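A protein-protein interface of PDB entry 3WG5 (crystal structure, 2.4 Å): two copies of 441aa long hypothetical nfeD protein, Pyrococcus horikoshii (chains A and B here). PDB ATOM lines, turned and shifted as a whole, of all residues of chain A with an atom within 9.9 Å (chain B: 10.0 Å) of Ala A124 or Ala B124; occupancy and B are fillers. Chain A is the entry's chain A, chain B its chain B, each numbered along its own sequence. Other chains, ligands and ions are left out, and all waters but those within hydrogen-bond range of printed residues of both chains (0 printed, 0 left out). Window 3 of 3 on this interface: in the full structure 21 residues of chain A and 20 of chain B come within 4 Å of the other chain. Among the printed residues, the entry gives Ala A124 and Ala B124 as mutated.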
ATOM      1  N   PRO A 108     -28.085  38.486  25.059  1.00  0.00           N
ATOM      2  CA  PRO A 108     -27.702  37.105  25.333  1.00  0.00           C
ATOM      3  C   PRO A 108     -26.330  36.780  24.763  1.00  0.00           C
ATOM      4  O   PRO A 108     -26.032  37.145  23.620  1.00  0.00           O
ATOM      5  CB  PRO A 108     -28.783  36.283  24.620  1.00  0.00           C
ATOM      6  CG  PRO A 108     -29.332  37.199  23.583  1.00  0.00           C
ATOM      7  CD  PRO A 108     -29.259  38.572  24.173  1.00  0.00           C
ATOM      8  N   LEU A 110     -23.184  33.469  24.595  1.00  0.00           N
ATOM      9  CA  LEU A 110     -22.759  32.109  24.862  1.00  0.00           C
ATOM     10  C   LEU A 110     -21.787  32.050  26.038  1.00  0.00           C
ATOM     11  O   LEU A 110     -21.591  30.989  26.622  1.00  0.00           O
ATOM     12  CB  LEU A 110     -22.147  31.464  23.610  1.00  0.00           C
ATOM     13  CG  LEU A 110     -23.082  30.635  22.725  1.00  0.00           C
ATOM     14  CD1 LEU A 110     -22.357  30.226  21.453  1.00  0.00           C
ATOM     15  CD2 LEU A 110     -23.610  29.399  23.460  1.00  0.00           C
ATOM     16  N   GLU A 120     -20.222  35.740  21.549  1.00  0.00           N
ATOM     17  CA  GLU A 120     -21.570  36.129  21.141  1.00  0.00           C
ATOM     18  C   GLU A 120     -22.417  34.918  20.749  1.00  0.00           C
ATOM     19  O   GLU A 120     -21.892  33.856  20.397  1.00  0.00           O
ATOM     20  CB  GLU A 120     -21.528  37.142  19.987  1.00  0.00           C
ATOM     21  CG  GLU A 120     -20.792  38.451  20.285  1.00  0.00           C
ATOM     22  CD  GLU A 120     -21.593  39.433  21.129  1.00  0.00           C
ATOM     23  OE1 GLU A 120     -22.794  39.191  21.384  1.00  0.00           O
ATOM     24  OE2 GLU A 120     -21.014  40.463  21.540  1.00  0.00           O
ATOM     25  N   ALA A 121     -23.731  35.087  20.827  1.00  0.00           N
ATOM     26  CA  ALA A 121     -24.664  34.048  20.433  1.00  0.00           C
ATOM     27  C   ALA A 121     -24.958  34.170  18.937  1.00  0.00           C
ATOM     28  O   ALA A 121     -24.753  35.236  18.357  1.00  0.00           O
ATOM     29  CB  ALA A 121     -25.951  34.171  21.250  1.00  0.00           C
ATOM     30  N   PRO A 122     -25.419  33.075  18.298  1.00  0.00           N
ATOM     31  CA  PRO A 122     -25.926  33.177  16.921  1.00  0.00           C
ATOM     32  C   PRO A 122     -27.034  34.226  16.821  1.00  0.00           C
ATOM     33  O   PRO A 122     -27.808  34.377  17.766  1.00  0.00           O
ATOM     34  CB  PRO A 122     -26.495  31.783  16.645  1.00  0.00           C
ATOM     35  CG  PRO A 122     -25.686  30.875  17.514  1.00  0.00           C
ATOM     36  CD  PRO A 122     -25.298  31.672  18.744  1.00  0.00           C
ATOM     37  N   PRO A 123     -27.106  34.955  15.690  1.00  0.00           N
ATOM     38  CA  PRO A 123     -28.075  36.052  15.573  1.00  0.00           C
ATOM     39  C   PRO A 123     -29.498  35.632  15.949  1.00  0.00           C
ATOM     40  O   PRO A 123     -30.195  36.389  16.617  1.00  0.00           O
ATOM     41  CB  PRO A 123     -27.997  36.443  14.090  1.00  0.00           C
ATOM     42  CG  PRO A 123     -26.643  36.000  13.652  1.00  0.00           C
ATOM     43  CD  PRO A 123     -26.346  34.756  14.439  1.00  0.00           C
ATOM     44  N   ALA A 124     -29.897  34.424  15.549  1.00  0.00           N
ATOM     45  CA  ALA A 124     -31.250  33.915  15.800  1.00  0.00           C
ATOM     46  C   ALA A 124     -31.603  33.752  17.288  1.00  0.00           C
ATOM     47  O   ALA A 124     -32.752  33.984  17.681  1.00  0.00           O
ATOM     48  CB  ALA A 124     -31.493  32.612  15.031  1.00  0.00           C
ATOM     49  N   ILE A 125     -30.631  33.372  18.111  1.00  0.00           N
ATOM     50  CA  ILE A 125     -30.868  33.301  19.563  1.00  0.00           C
ATOM     51  C   ILE A 125     -30.981  34.689  20.237  1.00  0.00           C
ATOM     52  O   ILE A 125     -31.665  34.850  21.255  1.00  0.00           O
ATOM     53  CB  ILE A 125     -29.910  32.318  20.296  1.00  0.00           C
ATOM     54  CG1 ILE A 125     -29.554  32.815  21.698  1.00  0.00           C
ATOM     55  CG2 ILE A 125     -28.665  32.073  19.495  1.00  0.00           C
ATOM     56  CD1 ILE A 125     -29.346  31.698  22.657  1.00  0.00           C
ATOM     57  N   THR A 126     -30.330  35.688  19.649  1.00  0.00           N
ATOM     58  CA  THR A 126     -30.607  37.069  20.004  1.00  0.00           C
ATOM     59  C   THR A 126     -32.083  37.370  19.727  1.00  0.00           C
ATOM     60  O   THR A 126     -32.774  37.937  20.583  1.00  0.00           O
ATOM     61  CB  THR A 126     -29.647  38.037  19.282  1.00  0.00           C
ATOM     62  OG1 THR A 126     -28.330  37.860  19.815  1.00  0.00           O
ATOM     63  CG2 THR A 126     -30.059  39.493  19.453  1.00  0.00           C
ATOM     64  N   ASN A 127     -32.582  36.964  18.560  1.00  0.00           N
ATOM     65  CA  ASN A 127     -34.000  37.157  18.230  1.00  0.00           C
ATOM     66  C   ASN A 127     -34.956  36.403  19.178  1.00  0.00           C
ATOM     67  O   ASN A 127     -36.062  36.869  19.446  1.00  0.00           O
ATOM     68  CB  ASN A 127     -34.292  36.781  16.768  1.00  0.00           C
ATOM     69  CG  ASN A 127     -33.458  37.577  15.766  1.00  0.00           C
ATOM     70  OD1 ASN A 127     -33.372  38.806  15.829  1.00  0.00           O
ATOM     71  ND2 ASN A 127     -32.856  36.870  14.820  1.00  0.00           N
ATOM     72  N   TYR A 128     -34.527  35.243  19.672  1.00  0.00           N
ATOM     73  CA  TYR A 128     -35.296  34.484  20.664  1.00  0.00           C
ATOM     74  C   TYR A 128     -35.443  35.283  21.975  1.00  0.00           C
ATOM     75  O   TYR A 128     -36.558  35.475  22.474  1.00  0.00           O
ATOM     76  CB  TYR A 128     -34.659  33.105  20.907  1.00  0.00           C
ATOM     77  CG  TYR A 128     -35.308  32.256  21.989  1.00  0.00           C
ATOM     78  CD1 TYR A 128     -36.202  31.224  21.664  1.00  0.00           C
ATOM     79  CD2 TYR A 128     -35.014  32.467  23.333  1.00  0.00           C
ATOM     80  CE1 TYR A 128     -36.783  30.430  22.663  1.00  0.00           C
ATOM     81  CE2 TYR A 128     -35.593  31.694  24.327  1.00  0.00           C
ATOM     82  CZ  TYR A 128     -36.471  30.677  23.984  1.00  0.00           C
ATOM     83  OH  TYR A 128     -37.029  29.922  24.986  1.00  0.00           O
ATOM     84  N   PHE A 129     -34.330  35.769  22.512  1.00  0.00           N
ATOM     85  CA  PHE A 129     -34.390  36.601  23.721  1.00  0.00           C
ATOM     86  C   PHE A 129     -35.090  37.954  23.536  1.00  0.00           C
ATOM     87  O   PHE A 129     -35.674  38.487  24.482  1.00  0.00           O
ATOM     88  CB  PHE A 129     -33.014  36.732  24.369  1.00  0.00           C
ATOM     89  CG  PHE A 129     -32.621  35.511  25.149  1.00  0.00           C
ATOM     90  CD1 PHE A 129     -31.950  34.464  24.532  1.00  0.00           C
ATOM     91  CD2 PHE A 129     -32.975  35.384  26.490  1.00  0.00           C
ATOM     92  CE1 PHE A 129     -31.603  33.325  25.245  1.00  0.00           C
ATOM     93  CE2 PHE A 129     -32.631  34.255  27.207  1.00  0.00           C
ATOM     94  CZ  PHE A 129     -31.945  33.220  26.586  1.00  0.00           C
ATOM     95  N   ILE A 130     -35.064  38.481  22.314  1.00  0.00           N
ATOM     96  CA  ILE A 130     -35.839  39.674  21.993  1.00  0.00           C
ATOM     97  C   ILE A 130     -37.329  39.361  22.141  1.00  0.00           C
ATOM     98  O   ILE A 130     -38.051  40.087  22.835  1.00  0.00           O
ATOM     99  CB  ILE A 130     -35.511  40.233  20.575  1.00  0.00           C
ATOM    100  CG1 ILE A 130     -34.134  40.906  20.578  1.00  0.00           C
ATOM    101  CG2 ILE A 130     -36.590  41.224  20.098  1.00  0.00           C
ATOM    102  CD1 ILE A 130     -33.579  41.191  19.166  1.00  0.00           C
ATOM    103  N   ALA A 131     -37.773  38.274  21.507  1.00  0.00           N
ATOM    104  CA  ALA A 131     -39.166  37.826  21.624  1.00  0.00           C
ATOM    105  C   ALA A 131     -39.548  37.632  23.095  1.00  0.00           C
ATOM    106  O   ALA A 131     -40.587  38.131  23.542  1.00  0.00           O
ATOM    107  CB  ALA A 131     -39.396  36.537  20.832  1.00  0.00           C
ATOM    108  N   TYR A 132     -38.687  36.941  23.843  1.00  0.00           N
ATOM    109  CA  TYR A 132     -38.936  36.658  25.256  1.00  0.00           C
ATOM    110  C   TYR A 132     -39.062  37.945  26.100  1.00  0.00           C
ATOM    111  O   TYR A 132     -40.017  38.099  26.858  1.00  0.00           O
ATOM    112  CB  TYR A 132     -37.856  35.709  25.802  1.00  0.00           C
ATOM    113  CG  TYR A 132     -38.055  35.294  27.244  1.00  0.00           C
ATOM    114  CD1 TYR A 132     -39.043  34.368  27.608  1.00  0.00           C
ATOM    115  CD2 TYR A 132     -37.249  35.814  28.242  1.00  0.00           C
ATOM    116  CE1 TYR A 132     -39.223  33.987  28.938  1.00  0.00           C
ATOM    117  CE2 TYR A 132     -37.418  35.442  29.574  1.00  0.00           C
ATOM    118  CZ  TYR A 132     -38.396  34.534  29.917  1.00  0.00           C
ATOM    119  OH  TYR A 132     -38.545  34.197  31.244  1.00  0.00           O
ATOM    120  N   ILE A 151     -31.420  44.839  24.752  1.00  0.00           N
ATOM    121  CA  ILE A 151     -30.655  43.823  24.031  1.00  0.00           C
ATOM    122  C   ILE A 151     -29.932  44.431  22.825  1.00  0.00           C
ATOM    123  O   ILE A 151     -28.706  44.392  22.760  1.00  0.00           O
ATOM    124  CB  ILE A 151     -31.552  42.632  23.588  1.00  0.00           C
ATOM    125  CG1 ILE A 151     -32.000  41.819  24.816  1.00  0.00           C
ATOM    126  CG2 ILE A 151     -30.818  41.734  22.575  1.00  0.00           C
ATOM    127  CD1 ILE A 151     -33.180  40.860  24.564  1.00  0.00           C
ATOM    128  N   PRO B 108     -28.806  19.731  23.122  1.00  0.00           N
ATOM    129  CA  PRO B 108     -28.788  20.922  23.976  1.00  0.00           C
ATOM    130  C   PRO B 108     -30.191  21.344  24.411  1.00  0.00           C
ATOM    131  O   PRO B 108     -31.151  21.171  23.659  1.00  0.00           O
ATOM    132  CB  PRO B 108     -28.149  21.991  23.089  1.00  0.00           C
ATOM    133  CG  PRO B 108     -28.353  21.521  21.694  1.00  0.00           C
ATOM    134  CD  PRO B 108     -28.430  20.027  21.728  1.00  0.00           C
ATOM    135  N   LEU B 110     -32.141  24.710  26.921  1.00  0.00           N
ATOM    136  CA  LEU B 110     -31.898  25.958  27.637  1.00  0.00           C
ATOM    137  C   LEU B 110     -31.757  25.671  29.128  1.00  0.00           C
ATOM    138  O   LEU B 110     -31.073  26.406  29.834  1.00  0.00           O
ATOM    139  CB  LEU B 110     -32.981  27.001  27.359  1.00  0.00           C
ATOM    140  CG  LEU B 110     -33.019  27.654  25.972  1.00  0.00           C
ATOM    141  CD1 LEU B 110     -34.073  28.749  25.939  1.00  0.00           C
ATOM    142  CD2 LEU B 110     -31.681  28.229  25.567  1.00  0.00           C
ATOM    143  N   GLU B 120     -36.918  24.075  26.053  1.00  0.00           N
ATOM    144  CA  GLU B 120     -36.396  23.670  24.753  1.00  0.00           C
ATOM    145  C   GLU B 120     -35.327  24.631  24.243  1.00  0.00           C
ATOM    146  O   GLU B 120     -35.385  25.835  24.500  1.00  0.00           O
ATOM    147  CB  GLU B 120     -37.534  23.548  23.735  1.00  0.00           C
ATOM    148  CG  GLU B 120     -37.217  22.638  22.539  1.00  0.00           C
ATOM    149  CD  GLU B 120     -38.451  22.264  21.720  1.00  0.00           C
ATOM    150  OE1 GLU B 120     -39.275  23.156  21.424  1.00  0.00           O
ATOM    151  OE2 GLU B 120     -38.589  21.075  21.362  1.00  0.00           O
ATOM    152  N   ALA B 121     -34.344  24.089  23.538  1.00  0.00           N
ATOM    153  CA  ALA B 121     -33.372  24.914  22.842  1.00  0.00           C
ATOM    154  C   ALA B 121     -33.964  25.317  21.504  1.00  0.00           C
ATOM    155  O   ALA B 121     -34.541  24.474  20.806  1.00  0.00           O
ATOM    156  CB  ALA B 121     -32.075  24.159  22.641  1.00  0.00           C
ATOM    157  N   PRO B 122     -33.836  26.608  21.136  1.00  0.00           N
ATOM    158  CA  PRO B 122     -34.266  27.018  19.798  1.00  0.00           C
ATOM    159  C   PRO B 122     -33.426  26.288  18.742  1.00  0.00           C
ATOM    160  O   PRO B 122     -32.270  25.961  19.012  1.00  0.00           O
ATOM    161  CB  PRO B 122     -33.975  28.526  19.775  1.00  0.00           C
ATOM    162  CG  PRO B 122     -33.730  28.919  21.202  1.00  0.00           C
ATOM    163  CD  PRO B 122     -33.205  27.712  21.886  1.00  0.00           C
ATOM    164  N   PRO B 123     -34.001  26.025  17.551  1.00  0.00           N
ATOM    165  CA  PRO B 123     -33.299  25.303  16.478  1.00  0.00           C
ATOM    166  C   PRO B 123     -31.878  25.810  16.151  1.00  0.00           C
ATOM    167  O   PRO B 123     -30.999  25.000  15.845  1.00  0.00           O
ATOM    168  CB  PRO B 123     -34.227  25.489  15.277  1.00  0.00           C
ATOM    169  CG  PRO B 123     -35.580  25.593  15.884  1.00  0.00           C
ATOM    170  CD  PRO B 123     -35.393  26.342  17.174  1.00  0.00           C
ATOM    171  N   ALA B 124     -31.658  27.123  16.217  1.00  0.00           N
ATOM    172  CA  ALA B 124     -30.343  27.695  15.917  1.00  0.00           C
ATOM    173  C   ALA B 124     -29.249  27.108  16.820  1.00  0.00           C
ATOM    174  O   ALA B 124     -28.261  26.570  16.319  1.00  0.00           O
ATOM    175  CB  ALA B 124     -30.374  29.213  16.009  1.00  0.00           C
ATOM    176  N   ILE B 125     -29.446  27.204  18.136  1.00  0.00           N
ATOM    177  CA  ILE B 125     -28.605  26.526  19.128  1.00  0.00           C
ATOM    178  C   ILE B 125     -28.343  25.057  18.787  1.00  0.00           C
ATOM    179  O   ILE B 125     -27.208  24.595  18.843  1.00  0.00           O
ATOM    180  CB  ILE B 125     -29.228  26.607  20.551  1.00  0.00           C
ATOM    181  CG1 ILE B 125     -29.105  28.024  21.141  1.00  0.00           C
ATOM    182  CG2 ILE B 125     -28.619  25.553  21.483  1.00  0.00           C
ATOM    183  CD1 ILE B 125     -27.667  28.505  21.436  1.00  0.00           C
ATOM    184  N   THR B 126     -29.399  24.329  18.446  1.00  0.00           N
ATOM    185  CA  THR B 126     -29.282  22.917  18.094  1.00  0.00           C
ATOM    186  C   THR B 126     -28.361  22.728  16.884  1.00  0.00           C
ATOM    187  O   THR B 126     -27.409  21.945  16.951  1.00  0.00           O
ATOM    188  CB  THR B 126     -30.676  22.275  17.874  1.00  0.00           C
ATOM    189  OG1 THR B 126     -31.406  22.319  19.109  1.00  0.00           O
ATOM    190  CG2 THR B 126     -30.553  20.818  17.401  1.00  0.00           C
ATOM    191  N   ASN B 127     -28.642  23.466  15.808  1.00  0.00           N
ATOM    192  CA  ASN B 127     -27.821  23.460  14.595  1.00  0.00           C
ATOM    193  C   ASN B 127     -26.387  23.906  14.855  1.00  0.00           C
ATOM    194  O   ASN B 127     -25.456  23.393  14.251  1.00  0.00           O
ATOM    195  CB  ASN B 127     -28.444  24.353  13.511  1.00  0.00           C
ATOM    196  CG  ASN B 127     -29.788  23.838  13.022  1.00  0.00           C
ATOM    197  OD1 ASN B 127     -30.079  22.640  13.084  1.00  0.00           O
ATOM    198  ND2 ASN B 127     -30.617  24.748  12.529  1.00  0.00           N
ATOM    199  N   TYR B 128     -26.220  24.864  15.757  1.00  0.00           N
ATOM    200  CA  TYR B 128     -24.904  25.362  16.112  1.00  0.00           C
ATOM    201  C   TYR B 128     -24.070  24.243  16.758  1.00  0.00           C
ATOM    202  O   TYR B 128     -22.880  24.093  16.447  1.00  0.00           O
ATOM    203  CB  TYR B 128     -25.048  26.565  17.042  1.00  0.00           C
ATOM    204  CG  TYR B 128     -23.761  27.142  17.599  1.00  0.00           C
ATOM    205  CD1 TYR B 128     -23.148  28.245  17.002  1.00  0.00           C
ATOM    206  CD2 TYR B 128     -23.175  26.607  18.739  1.00  0.00           C
ATOM    207  CE1 TYR B 128     -21.972  28.784  17.518  1.00  0.00           C
ATOM    208  CE2 TYR B 128     -22.007  27.131  19.253  1.00  0.00           C
ATOM    209  CZ  TYR B 128     -21.408  28.226  18.640  1.00  0.00           C
ATOM    210  OH  TYR B 128     -20.248  28.758  19.177  1.00  0.00           O
ATOM    211  N   PHE B 129     -24.696  23.450  17.635  1.00  0.00           N
ATOM    212  CA  PHE B 129     -23.958  22.387  18.311  1.00  0.00           C
ATOM    213  C   PHE B 129     -23.741  21.157  17.452  1.00  0.00           C
ATOM    214  O   PHE B 129     -22.721  20.486  17.601  1.00  0.00           O
ATOM    215  CB  PHE B 129     -24.532  22.077  19.693  1.00  0.00           C
ATOM    216  CG  PHE B 129     -24.185  23.121  20.704  1.00  0.00           C
ATOM    217  CD1 PHE B 129     -25.012  24.221  20.897  1.00  0.00           C
ATOM    218  CD2 PHE B 129     -22.990  23.050  21.400  1.00  0.00           C
ATOM    219  CE1 PHE B 129     -24.668  25.220  21.807  1.00  0.00           C
ATOM    220  CE2 PHE B 129     -22.637  24.031  22.312  1.00  0.00           C
ATOM    221  CZ  PHE B 129     -23.478  25.123  22.520  1.00  0.00           C
ATOM    222  N   ILE B 130     -24.676  20.895  16.535  1.00  0.00           N
ATOM    223  CA  ILE B 130     -24.495  19.885  15.493  1.00  0.00           C
ATOM    224  C   ILE B 130     -23.220  20.175  14.695  1.00  0.00           C
ATOM    225  O   ILE B 130     -22.364  19.299  14.568  1.00  0.00           O
ATOM    226  CB  ILE B 130     -25.722  19.774  14.549  1.00  0.00           C
ATOM    227  CG1 ILE B 130     -26.894  19.090  15.265  1.00  0.00           C
ATOM    228  CG2 ILE B 130     -25.379  18.969  13.283  1.00  0.00           C
ATOM    229  CD1 ILE B 130     -28.243  19.177  14.506  1.00  0.00           C
ATOM    230  N   ALA B 131     -23.083  21.404  14.199  1.00  0.00           N
ATOM    231  CA  ALA B 131     -21.905  21.812  13.422  1.00  0.00           C
ATOM    232  C   ALA B 131     -20.622  21.711  14.252  1.00  0.00           C
ATOM    233  O   ALA B 131     -19.597  21.242  13.762  1.00  0.00           O
ATOM    234  CB  ALA B 131     -22.080  23.237  12.869  1.00  0.00           C
ATOM    235  N   TYR B 132     -20.693  22.139  15.508  1.00  0.00           N
ATOM    236  CA  TYR B 132     -19.547  22.077  16.424  1.00  0.00           C
ATOM    237  C   TYR B 132     -19.090  20.633  16.719  1.00  0.00           C
ATOM    238  O   TYR B 132     -17.898  20.319  16.629  1.00  0.00           O
ATOM    239  CB  TYR B 132     -19.876  22.826  17.727  1.00  0.00           C
ATOM    240  CG  TYR B 132     -18.724  22.946  18.711  1.00  0.00           C
ATOM    241  CD1 TYR B 132     -17.575  23.678  18.392  1.00  0.00           C
ATOM    242  CD2 TYR B 132     -18.795  22.343  19.971  1.00  0.00           C
ATOM    243  CE1 TYR B 132     -16.524  23.795  19.299  1.00  0.00           C
ATOM    244  CE2 TYR B 132     -17.758  22.454  20.885  1.00  0.00           C
ATOM    245  CZ  TYR B 132     -16.626  23.182  20.546  1.00  0.00           C
ATOM    246  OH  TYR B 132     -15.588  23.291  21.447  1.00  0.00           O
ATOM    247  N   ILE B 151     -26.679  14.219  19.461  1.00  0.00           N
ATOM    248  CA  ILE B 151     -27.597  15.343  19.583  1.00  0.00           C
ATOM    249  C   ILE B 151     -28.980  14.984  19.020  1.00  0.00           C
ATOM    250  O   ILE B 151     -29.968  14.988  19.748  1.00  0.00           O
ATOM    251  CB  ILE B 151     -27.035  16.624  18.888  1.00  0.00           C
ATOM    252  CG1 ILE B 151     -25.774  17.130  19.621  1.00  0.00           C
ATOM    253  CG2 ILE B 151     -28.101  17.721  18.834  1.00  0.00           C
ATOM    254  CD1 ILE B 151     -25.079  18.294  18.962  1.00  0.00           C
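Leu A110 touches Tyr B128.
CD1 of Tyr B128 touches CG of Pro A122, at 3.7 Å.
Ala B124 touches Ala A124.
Ile A125 touches Ile B125.
Tyr A128 touches Leu B110.
CD1 of Tyr A128 touches CG of Pro B122, at 3.4 Å.
Of the printed residues of chain B, Pro A122 touches Tyr B128.
Of chain B, only Ala B124 (3.7 Å) comes within 4 Å of Ala A124.
No residue of chain B comes within 4 Å of Asn A127.
Of the printed residues of chain B, Tyr A128 touches Leu B110 (3.3 Å) and Pro B122 (3.4 Å).
Ile A151 touches none of the printed residues of chain B.
Printed residues of chain A within 4 Å of Pro B122: Tyr A128 (3.4 Å).
No residue of chain A comes within 4 Å of Pro B123.
Ala B124 touches just one residue of chain A: Ala A124 (3.7 Å).
Ile B125 touches one residue of chain A.
No residue of chain A comes within 4 Å of Asn B127.
The nearest printed residue of chain A that does not touch Leu B110 is Phe A129 (5.0 Å).
Among the printed residues, 6 pairs touch across the chains.
Leu A110 touches Tyr B128, and with the chains exchanged Tyr A128 touches Leu B110.
Pro A122 touches Tyr B128, and with the chains exchanged Tyr A128 touches Pro B122.
Ala B124 touches its own counterpart, Ala A124.
Ile A125 touches its own counterpart, Ile B125.
Positions printed for both chains: 108, 110, 120, 121, 122, 123, 124, 125, 126, 127, 128, 129, 130, 131, 132 and 151.
Of the 6 pairs that touch across the chains among the printed residues, 6 have their exchanged pair printed and touching as well.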
